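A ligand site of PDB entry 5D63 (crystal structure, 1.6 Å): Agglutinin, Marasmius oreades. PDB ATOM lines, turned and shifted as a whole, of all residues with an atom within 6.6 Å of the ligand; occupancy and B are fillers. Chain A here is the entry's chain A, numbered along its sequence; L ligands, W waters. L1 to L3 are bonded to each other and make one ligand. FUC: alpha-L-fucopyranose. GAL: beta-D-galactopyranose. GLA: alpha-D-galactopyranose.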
ATOM      1  N   HIS A   9      -2.353  -7.148  -4.180  1.00  0.00           N
ATOM      2  CA  HIS A   9      -2.265  -5.768  -4.681  1.00  0.00           C
ATOM      3  C   HIS A   9      -2.011  -5.916  -6.167  1.00  0.00           C
ATOM      4  O   HIS A   9      -1.063  -6.619  -6.557  1.00  0.00           O
ATOM      5  CB  HIS A   9      -1.107  -5.079  -3.991  1.00  0.00           C
ATOM      6  CG  HIS A   9      -0.995  -3.624  -4.324  1.00  0.00           C
ATOM      7  ND1 HIS A   9      -0.010  -3.103  -5.174  1.00  0.00           N
ATOM      8  CD2 HIS A   9      -1.801  -2.580  -3.999  1.00  0.00           C
ATOM      9  CE1 HIS A   9      -0.231  -1.829  -5.345  1.00  0.00           C
ATOM     10  NE2 HIS A   9      -1.286  -1.473  -4.619  1.00  0.00           N
ATOM     11  N   ASP A  20      -7.956   0.085  -7.920  1.00  0.00           N
ATOM     12  CA  ASP A  20      -8.354   0.806  -6.740  1.00  0.00           C
ATOM     13  C   ASP A  20      -9.904   0.979  -6.769  1.00  0.00           C
ATOM     14  O   ASP A  20     -10.535   1.397  -7.718  1.00  0.00           O
ATOM     15  CB  ASP A  20      -7.567   2.121  -6.785  1.00  0.00           C
ATOM     16  CG  ASP A  20      -7.865   3.094  -5.604  1.00  0.00           C
ATOM     17  OD1 ASP A  20      -9.046   3.497  -5.365  1.00  0.00           O
ATOM     18  OD2 ASP A  20      -6.902   3.498  -4.894  1.00  0.00           O
ATOM     19  N   LEU A  21     -10.532   0.630  -5.676  1.00  0.00           N
ATOM     20  CA  LEU A  21     -11.965   0.873  -5.502  1.00  0.00           C
ATOM     21  C   LEU A  21     -12.122   2.264  -4.972  1.00  0.00           C
ATOM     22  O   LEU A  21     -11.658   2.613  -3.836  1.00  0.00           O
ATOM     23  CB  LEU A  21     -12.546  -0.117  -4.499  1.00  0.00           C
ATOM     24  CG  LEU A  21     -14.019   0.056  -4.223  1.00  0.00           C
ATOM     25  CD1 LEU A  21     -14.931  -0.143  -5.460  1.00  0.00           C
ATOM     26  CD2 LEU A  21     -14.514  -0.913  -3.131  1.00  0.00           C
ATOM     27  N   LYS A  22     -12.718   3.136  -5.782  1.00  0.00           N
ATOM     28  CA  LYS A  22     -12.583   4.592  -5.552  1.00  0.00           C
ATOM     29  C   LYS A  22     -13.163   4.988  -4.177  1.00  0.00           C
ATOM     30  O   LYS A  22     -14.332   4.710  -3.844  1.00  0.00           O
ATOM     31  CB  LYS A  22     -13.239   5.363  -6.692  1.00  0.00           C
ATOM     32  CG  LYS A  22     -12.664   6.778  -6.836  1.00  0.00           C
ATOM     33  CD  LYS A  22     -13.301   7.601  -7.961  1.00  0.00           C
ATOM     34  CE  LYS A  22     -12.640   9.009  -7.948  1.00  0.00           C
ATOM     35  NZ  LYS A  22     -13.012   9.693  -9.314  1.00  0.00           N
ATOM     36  N   ASP A  23     -12.373   5.715  -3.387  1.00  0.00           N
ATOM     37  CA  ASP A  23     -12.697   6.104  -2.020  1.00  0.00           C
ATOM     38  C   ASP A  23     -13.062   4.974  -1.082  1.00  0.00           C
ATOM     39  O   ASP A  23     -13.566   5.197  -0.015  1.00  0.00           O
ATOM     40  CB  ASP A  23     -13.787   7.159  -2.042  1.00  0.00           C
ATOM     41  CG  ASP A  23     -13.700   8.114  -0.837  1.00  0.00           C
ATOM     42  OD1 ASP A  23     -12.586   8.427  -0.357  1.00  0.00           O
ATOM     43  OD2 ASP A  23     -14.800   8.432  -0.298  1.00  0.00           O
ATOM     44  N   GLY A  24     -12.699   3.758  -1.429  1.00  0.00           N
ATOM     45  CA  GLY A  24     -13.025   2.568  -0.629  1.00  0.00           C
ATOM     46  C   GLY A  24     -14.516   2.412  -0.463  1.00  0.00           C
ATOM     47  O   GLY A  24     -14.925   1.671   0.433  1.00  0.00           O
ATOM     48  N   VAL A  33     -10.840   1.929 -10.452  1.00  0.00           N
ATOM     49  CA  VAL A  33     -10.036   2.805 -11.271  1.00  0.00           C
ATOM     50  C   VAL A  33      -8.558   2.503 -11.107  1.00  0.00           C
ATOM     51  O   VAL A  33      -8.126   1.895 -10.110  1.00  0.00           O
ATOM     52  CB  VAL A  33     -10.203   4.313 -10.889  1.00  0.00           C
ATOM     53  CG1 VAL A  33     -11.635   4.707 -11.264  1.00  0.00           C
ATOM     54  CG2 VAL A  33      -9.963   4.516  -9.419  1.00  0.00           C
ATOM     55  N   TRP A  35      -4.853   3.821  -9.961  1.00  0.00           N
ATOM     56  CA  TRP A  35      -4.434   4.853  -8.990  1.00  0.00           C
ATOM     57  C   TRP A  35      -2.965   4.517  -8.593  1.00  0.00           C
ATOM     58  O   TRP A  35      -2.646   3.358  -8.353  1.00  0.00           O
ATOM     59  CB  TRP A  35      -5.337   4.811  -7.764  1.00  0.00           C
ATOM     60  CG  TRP A  35      -5.402   6.140  -7.031  1.00  0.00           C
ATOM     61  CD1 TRP A  35      -4.453   6.681  -6.183  1.00  0.00           C
ATOM     62  CD2 TRP A  35      -6.447   7.122  -7.129  1.00  0.00           C
ATOM     63  NE1 TRP A  35      -4.835   7.926  -5.750  1.00  0.00           N
ATOM     64  CE2 TRP A  35      -6.052   8.243  -6.326  1.00  0.00           C
ATOM     65  CE3 TRP A  35      -7.635   7.189  -7.850  1.00  0.00           C
ATOM     66  CZ2 TRP A  35      -6.830   9.380  -6.197  1.00  0.00           C
ATOM     67  CZ3 TRP A  35      -8.398   8.355  -7.733  1.00  0.00           C
ATOM     68  CH2 TRP A  35      -7.976   9.445  -6.940  1.00  0.00           C
ATOM     69  N   GLN A  36      -2.176   5.525  -8.339  1.00  0.00           N
ATOM     70  CA  GLN A  36      -0.846   5.309  -7.851  1.00  0.00           C
ATOM     71  C   GLN A  36      -0.817   4.745  -6.458  1.00  0.00           C
ATOM     72  O   GLN A  36      -1.761   4.854  -5.728  1.00  0.00           O
ATOM     73  CB  GLN A  36      -0.016   6.598  -7.889  1.00  0.00           C
ATOM     74  CG  GLN A  36      -0.435   7.688  -6.928  1.00  0.00           C
ATOM     75  CD  GLN A  36       0.449   8.913  -7.112  1.00  0.00           C
ATOM     76  OE1 GLN A  36       1.642   8.874  -6.868  1.00  0.00           O
ATOM     77  NE2 GLN A  36      -0.118   9.941  -7.632  1.00  0.00           N
ATOM     78  N   PHE A  37       0.331   4.234  -6.042  1.00  0.00           N
ATOM     79  CA  PHE A  37       0.434   3.537  -4.771  1.00  0.00           C
ATOM     80  C   PHE A  37       1.802   3.742  -4.140  1.00  0.00           C
ATOM     81  O   PHE A  37       2.696   4.263  -4.793  1.00  0.00           O
ATOM     82  CB  PHE A  37       0.244   1.976  -4.942  1.00  0.00           C
ATOM     83  CG  PHE A  37       1.287   1.284  -5.788  1.00  0.00           C
ATOM     84  CD1 PHE A  37       1.141   1.202  -7.147  1.00  0.00           C
ATOM     85  CD2 PHE A  37       2.362   0.673  -5.201  1.00  0.00           C
ATOM     86  CE1 PHE A  37       2.089   0.563  -7.945  1.00  0.00           C
ATOM     87  CE2 PHE A  37       3.355   0.020  -5.980  1.00  0.00           C
ATOM     88  CZ  PHE A  37       3.171  -0.003  -7.337  1.00  0.00           C
ATOM     89  N   THR A  38       1.855   3.385  -2.869  1.00  0.00           N
ATOM     90  CA  THR A  38       3.151   3.537  -2.098  1.00  0.00           C
ATOM     91  C   THR A  38       3.572   2.155  -1.653  1.00  0.00           C
ATOM     92  O   THR A  38       2.866   1.470  -0.918  1.00  0.00           O
ATOM     93  CB  THR A  38       2.959   4.476  -0.854  1.00  0.00           C
ATOM     94  OG1 THR A  38       2.381   5.744  -1.299  1.00  0.00           O
ATOM     95  CG2 THR A  38       4.288   4.706  -0.206  1.00  0.00           C
ATOM     96  N   PRO A  39       4.734   1.693  -2.097  1.00  0.00           N
ATOM     97  CA  PRO A  39       5.196   0.343  -1.677  1.00  0.00           C
ATOM     98  C   PRO A  39       5.447   0.265  -0.195  1.00  0.00           C
ATOM     99  O   PRO A  39       5.727   1.271   0.450  1.00  0.00           O
ATOM    100  CB  PRO A  39       6.518   0.137  -2.399  1.00  0.00           C
ATOM    101  CG  PRO A  39       6.760   1.394  -3.135  1.00  0.00           C
ATOM    102  CD  PRO A  39       5.672   2.382  -2.980  1.00  0.00           C
ATOM    103  N   THR A  41       3.470  -0.106   2.304  1.00  0.00           N
ATOM    104  CA  THR A  41       2.403   0.504   3.087  1.00  0.00           C
ATOM    105  C   THR A  41       1.187  -0.373   2.955  1.00  0.00           C
ATOM    106  O   THR A  41       1.148  -1.199   2.050  1.00  0.00           O
ATOM    107  CB  THR A  41       1.972   1.924   2.656  1.00  0.00           C
ATOM    108  OG1 THR A  41       1.295   1.832   1.366  1.00  0.00           O
ATOM    109  CG2 THR A  41       3.116   2.870   2.614  1.00  0.00           C
ATOM    110  N   ILE A  42       0.216  -0.211   3.835  1.00  0.00           N
ATOM    111  CA  ILE A  42      -1.129  -0.660   3.531  1.00  0.00           C
ATOM    112  C   ILE A  42      -1.745   0.347   2.552  1.00  0.00           C
ATOM    113  O   ILE A  42      -1.978   1.521   2.905  1.00  0.00           O
ATOM    114  CB  ILE A  42      -2.015  -0.795   4.786  1.00  0.00           C
ATOM    115  CG1 ILE A  42      -1.441  -1.856   5.785  1.00  0.00           C
ATOM    116  CG2 ILE A  42      -3.496  -1.002   4.387  1.00  0.00           C
ATOM    117  CD1 ILE A  42      -1.226  -3.220   5.223  1.00  0.00           C
ATOM    118  N   ASN A  43      -2.061  -0.128   1.336  1.00  0.00           N
ATOM    119  CA  ASN A  43      -2.822   0.666   0.309  1.00  0.00           C
ATOM    120  C   ASN A  43      -4.285   0.358   0.474  1.00  0.00           C
ATOM    121  O   ASN A  43      -4.801  -0.673  -0.049  1.00  0.00           O
ATOM    122  CB  ASN A  43      -2.291   0.339  -1.107  1.00  0.00           C
ATOM    123  CG  ASN A  43      -0.905   0.912  -1.336  1.00  0.00           C
ATOM    124  OD1 ASN A  43      -0.736   2.119  -1.534  1.00  0.00           O
ATOM    125  ND2 ASN A  43       0.112   0.093  -1.225  1.00  0.00           N
ATOM    126  N   TRP A  44      -4.936   1.156   1.339  1.00  0.00           N
ATOM    127  CA  TRP A  44      -6.229   0.871   1.911  1.00  0.00           C
ATOM    128  C   TRP A  44      -7.335   0.524   0.921  1.00  0.00           C
ATOM    129  O   TRP A  44      -8.216  -0.327   1.241  1.00  0.00           O
ATOM    130  CB  TRP A  44      -6.674   2.042   2.818  1.00  0.00           C
ATOM    131  CG  TRP A  44      -5.967   2.059   4.112  1.00  0.00           C
ATOM    132  CD1 TRP A  44      -4.838   2.771   4.462  1.00  0.00           C
ATOM    133  CD2 TRP A  44      -6.290   1.239   5.247  1.00  0.00           C
ATOM    134  NE1 TRP A  44      -4.508   2.490   5.758  1.00  0.00           N
ATOM    135  CE2 TRP A  44      -5.343   1.526   6.246  1.00  0.00           C
ATOM    136  CE3 TRP A  44      -7.295   0.339   5.493  1.00  0.00           C
ATOM    137  CZ2 TRP A  44      -5.385   0.920   7.497  1.00  0.00           C
ATOM    138  CZ3 TRP A  44      -7.337  -0.276   6.721  1.00  0.00           C
ATOM    139  CH2 TRP A  44      -6.349  -0.013   7.695  1.00  0.00           C
ATOM    140  N   HIS A  45      -7.354   1.120  -0.273  1.00  0.00           N
ATOM    141  CA  HIS A  45      -8.420   0.831  -1.220  1.00  0.00           C
ATOM    142  C   HIS A  45      -8.070  -0.115  -2.319  1.00  0.00           C
ATOM    143  O   HIS A  45      -8.829  -0.332  -3.287  1.00  0.00           O
ATOM    144  CB  HIS A  45      -8.957   2.173  -1.809  1.00  0.00           C
ATOM    145  CG  HIS A  45      -9.358   3.164  -0.746  1.00  0.00           C
ATOM    146  ND1 HIS A  45      -9.385   4.539  -0.974  1.00  0.00           N
ATOM    147  CD2 HIS A  45      -9.799   2.975   0.500  1.00  0.00           C
ATOM    148  CE1 HIS A  45      -9.849   5.140   0.113  1.00  0.00           C
ATOM    149  NE2 HIS A  45     -10.084   4.233   1.034  1.00  0.00           N
ATOM    150  N   GLN A  46      -6.888  -0.737  -2.263  1.00  0.00           N
ATOM    151  CA  GLN A  46      -6.256  -1.460  -3.361  1.00  0.00           C
ATOM    152  C   GLN A  46      -5.899  -2.906  -3.018  1.00  0.00           C
ATOM    153  O   GLN A  46      -5.033  -3.484  -3.648  1.00  0.00           O
ATOM    154  CB  GLN A  46      -4.955  -0.748  -3.744  1.00  0.00           C
ATOM    155  CG  GLN A  46      -5.189   0.722  -4.112  1.00  0.00           C
ATOM    156  CD  GLN A  46      -3.917   1.467  -4.517  1.00  0.00           C
ATOM    157  OE1 GLN A  46      -2.778   0.971  -4.354  1.00  0.00           O
ATOM    158  NE2 GLN A  46      -4.091   2.719  -4.996  1.00  0.00           N
ATOM    159  N   PHE A  66     -11.156  -3.706   2.110  1.00  0.00           N
ATOM    160  CA  PHE A  66     -11.719  -2.565   2.865  1.00  0.00           C
ATOM    161  C   PHE A  66     -13.231  -2.479   2.766  1.00  0.00           C
ATOM    162  O   PHE A  66     -13.892  -2.379   3.810  1.00  0.00           O
ATOM    163  CB  PHE A  66     -11.102  -1.270   2.382  1.00  0.00           C
ATOM    164  CG  PHE A  66     -11.540  -0.065   3.160  1.00  0.00           C
ATOM    165  CD1 PHE A  66     -11.065   0.166   4.476  1.00  0.00           C
ATOM    166  CD2 PHE A  66     -12.506   0.796   2.650  1.00  0.00           C
ATOM    167  CE1 PHE A  66     -11.523   1.234   5.212  1.00  0.00           C
ATOM    168  CE2 PHE A  66     -12.888   1.934   3.346  1.00  0.00           C
ATOM    169  CZ  PHE A  66     -12.357   2.183   4.606  1.00  0.00           C
ATOM    170  N   ASP A 131      -4.337   9.228 -11.817  1.00  0.00           N
ATOM    171  CA  ASP A 131      -5.145   8.755 -10.711  1.00  0.00           C
ATOM    172  C   ASP A 131      -6.623   8.919 -11.070  1.00  0.00           C
ATOM    173  O   ASP A 131      -7.118  10.051 -11.393  1.00  0.00           O
ATOM    174  CB  ASP A 131      -4.821   9.504  -9.451  1.00  0.00           C
ATOM    175  CG  ASP A 131      -3.395   9.253  -8.966  1.00  0.00           C
ATOM    176  OD1 ASP A 131      -2.874   8.190  -9.264  1.00  0.00           O
ATOM    177  OD2 ASP A 131      -2.863  10.117  -8.154  1.00  0.00           O
HETATM  178  C1  FUC L   1      -4.768   7.380   1.000  1.00  0.00           C
HETATM  179  C2  FUC L   1      -4.127   8.523   1.788  1.00  0.00           C
HETATM  180  C3  FUC L   1      -5.201   9.175   2.703  1.00  0.00           C
HETATM  181  C4  FUC L   1      -5.862   8.096   3.552  1.00  0.00           C
HETATM  182  C5  FUC L   1      -6.516   7.057   2.612  1.00  0.00           C
HETATM  183  C6  FUC L   1      -7.201   5.950   3.397  1.00  0.00           C
HETATM  184  O2  FUC L   1      -3.624   9.464   0.839  1.00  0.00           O
HETATM  185  O3  FUC L   1      -4.426  10.056   3.549  1.00  0.00           O
HETATM  186  O4  FUC L   1      -4.992   7.443   4.519  1.00  0.00           O
HETATM  187  O5  FUC L   1      -5.506   6.425   1.789  1.00  0.00           O
HETATM  188  C1  GAL L   2      -7.698   8.030  -1.079  1.00  0.00           C
HETATM  189  C2  GAL L   2      -6.479   7.131  -0.762  1.00  0.00           C
HETATM  190  C3  GAL L   2      -5.685   6.855  -2.046  1.00  0.00           C
HETATM  191  C4  GAL L   2      -6.512   6.256  -3.147  1.00  0.00           C
HETATM  192  C5  GAL L   2      -7.838   7.084  -3.296  1.00  0.00           C
HETATM  193  C6  GAL L   2      -8.845   6.565  -4.334  1.00  0.00           C
HETATM  194  O1  GAL L   2      -8.540   7.988   0.069  1.00  0.00           O
HETATM  195  O2  GAL L   2      -5.667   8.006   0.083  1.00  0.00           O
HETATM  196  O3  GAL L   2      -4.538   6.023  -1.735  1.00  0.00           O
HETATM  197  O4  GAL L   2      -6.906   4.925  -2.770  1.00  0.00           O
HETATM  198  O5  GAL L   2      -8.507   7.272  -2.006  1.00  0.00           O
HETATM  199  O6  GAL L   2      -9.572   5.427  -3.819  1.00  0.00           O
HETATM  200  C1  GLA L   3      -3.637   5.756  -2.811  1.00  0.00           C
HETATM  201  C2  GLA L   3      -2.466   4.935  -2.218  1.00  0.00           C
HETATM  202  C3  GLA L   3      -1.462   5.803  -1.460  1.00  0.00           C
HETATM  203  C4  GLA L   3      -1.085   7.081  -2.251  1.00  0.00           C
HETATM  204  C5  GLA L   3      -2.379   7.829  -2.596  1.00  0.00           C
HETATM  205  C6  GLA L   3      -2.248   9.054  -3.400  1.00  0.00           C
HETATM  206  O2  GLA L   3      -2.826   3.838  -1.397  1.00  0.00           O
HETATM  207  O3  GLA L   3      -0.264   5.053  -1.067  1.00  0.00           O
HETATM  208  O4  GLA L   3      -0.424   6.687  -3.468  1.00  0.00           O
HETATM  209  O5  GLA L   3      -3.200   6.928  -3.449  1.00  0.00           O
HETATM  210  O6  GLA L   3      -3.540   9.667  -3.686  1.00  0.00           O
HETATM  211  O   HOH W   1      -0.979   9.127   0.294  1.00  0.00           O
HETATM  212  O   HOH W   2      -6.005  10.549   5.931  1.00  0.00           O
HETATM  213  O   HOH W   3      -3.541   3.919   1.480  1.00  0.00           O
HETATM  214  O   HOH W   4      -5.541   2.997  -1.339  1.00  0.00           O
HETATM  215  O   HOH W   5      -0.656   3.821   1.202  1.00  0.00           O
HETATM  216  O   HOH W   6      -4.823  10.673  -1.433  1.00  0.00           O
HETATM  217  O   HOH W   7      -2.863   5.711   3.622  1.00  0.00           O
HETATM  218  O   HOH W   8      -4.006  11.567  -5.885  1.00  0.00           O
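An oxygen (O6) of GAL L2 sits at hydrogen-bond distance from the side-chain carboxylate of Asp 20 (2.5 Å).
The side-chain amide oxygen of Asn 43 is in hydrogen-bond range of an oxygen (O2) of GLA L3 (2.7 Å).
N of Thr 38 is in hydrogen-bond range of O3 of GLA L3 (3.2 Å).
The side-chain hydroxyl of Thr 38 lies within hydrogen-bond range of an oxygen (O3) of GLA L3, at 2.7 Å.
N of Asp 23 lies within hydrogen-bond range of O6 of GAL L2 (2.8 Å).
A ring nitrogen (ND1) of His 45 sits at hydrogen-bond distance from an oxygen (O6) of GAL L2 (3.0 Å).
An oxygen (O5) of GLA L3 lies within hydrogen-bond range of the indole nitrogen (NE1) of Trp 35 (3.0 Å).
O of Gln 36 sits at hydrogen-bond distance from O4 of GLA L3 (3.2 Å).
NE2 of Gln 46 sits at hydrogen-bond distance from OD2 of Asp 20, at 2.9 Å.
O of Asp 20 is in hydrogen-bond range of N of Val 33.
ND2 of Asn 43 lies within hydrogen-bond range of O of Thr 38 (3.1 Å).
The backbone carbonyl oxygen of Thr 38 lies within hydrogen-bond range of the side-chain hydroxyl of Thr 41 (2.8 Å).
O of His 45 lies within hydrogen-bond range of N of Leu 21 (3.1 Å).
ND1 of His 45 lies within hydrogen-bond range of N of Gly 24 (3.4 Å).
NE2 of Gln 46 is in hydrogen-bond range of O of Gln 36.
The side-chain amide nitrogen (NE2) of Gln 36 sits at hydrogen-bond distance from the side-chain carboxylate (OD2) of Asp 131.
O of Leu 21 touches O6 of GAL L2 (3.5 Å).
CA of Lys 22 touches O6 of GAL L2 (3.6 Å).
CA of Phe 37 touches O4 of GLA L3 (3.5 Å).
CB of Trp 44 touches C6 of FUC L1 (3.99 Å).
NE2 of Gln 46 touches C1 of GLA L3 (3.8 Å).
Hydrophobic or aromatic side chains within 4 Å of the ligand: Trp 35, Trp 44 and His 45.
Water W5 lies within hydrogen-bond range of O3 of GLA L3 (2.6 Å), OG1 of Thr 41 (2.8 Å), O of Ile 42 (3.2 Å) and OD1 of Asn 43 (3.2 Å).
Water W4 lies within hydrogen-bond range of O4 of GAL L2, N of His 45 and N of Trp 44.
Water W8 bridges OD2 of Asp 131 and O6 of GLA L3.
Water W3 lies within hydrogen-bond range of O2 of GLA L3 (3.0 Å), N of Trp 44 (3.1 Å) and O of Ile 42 (3.2 Å).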
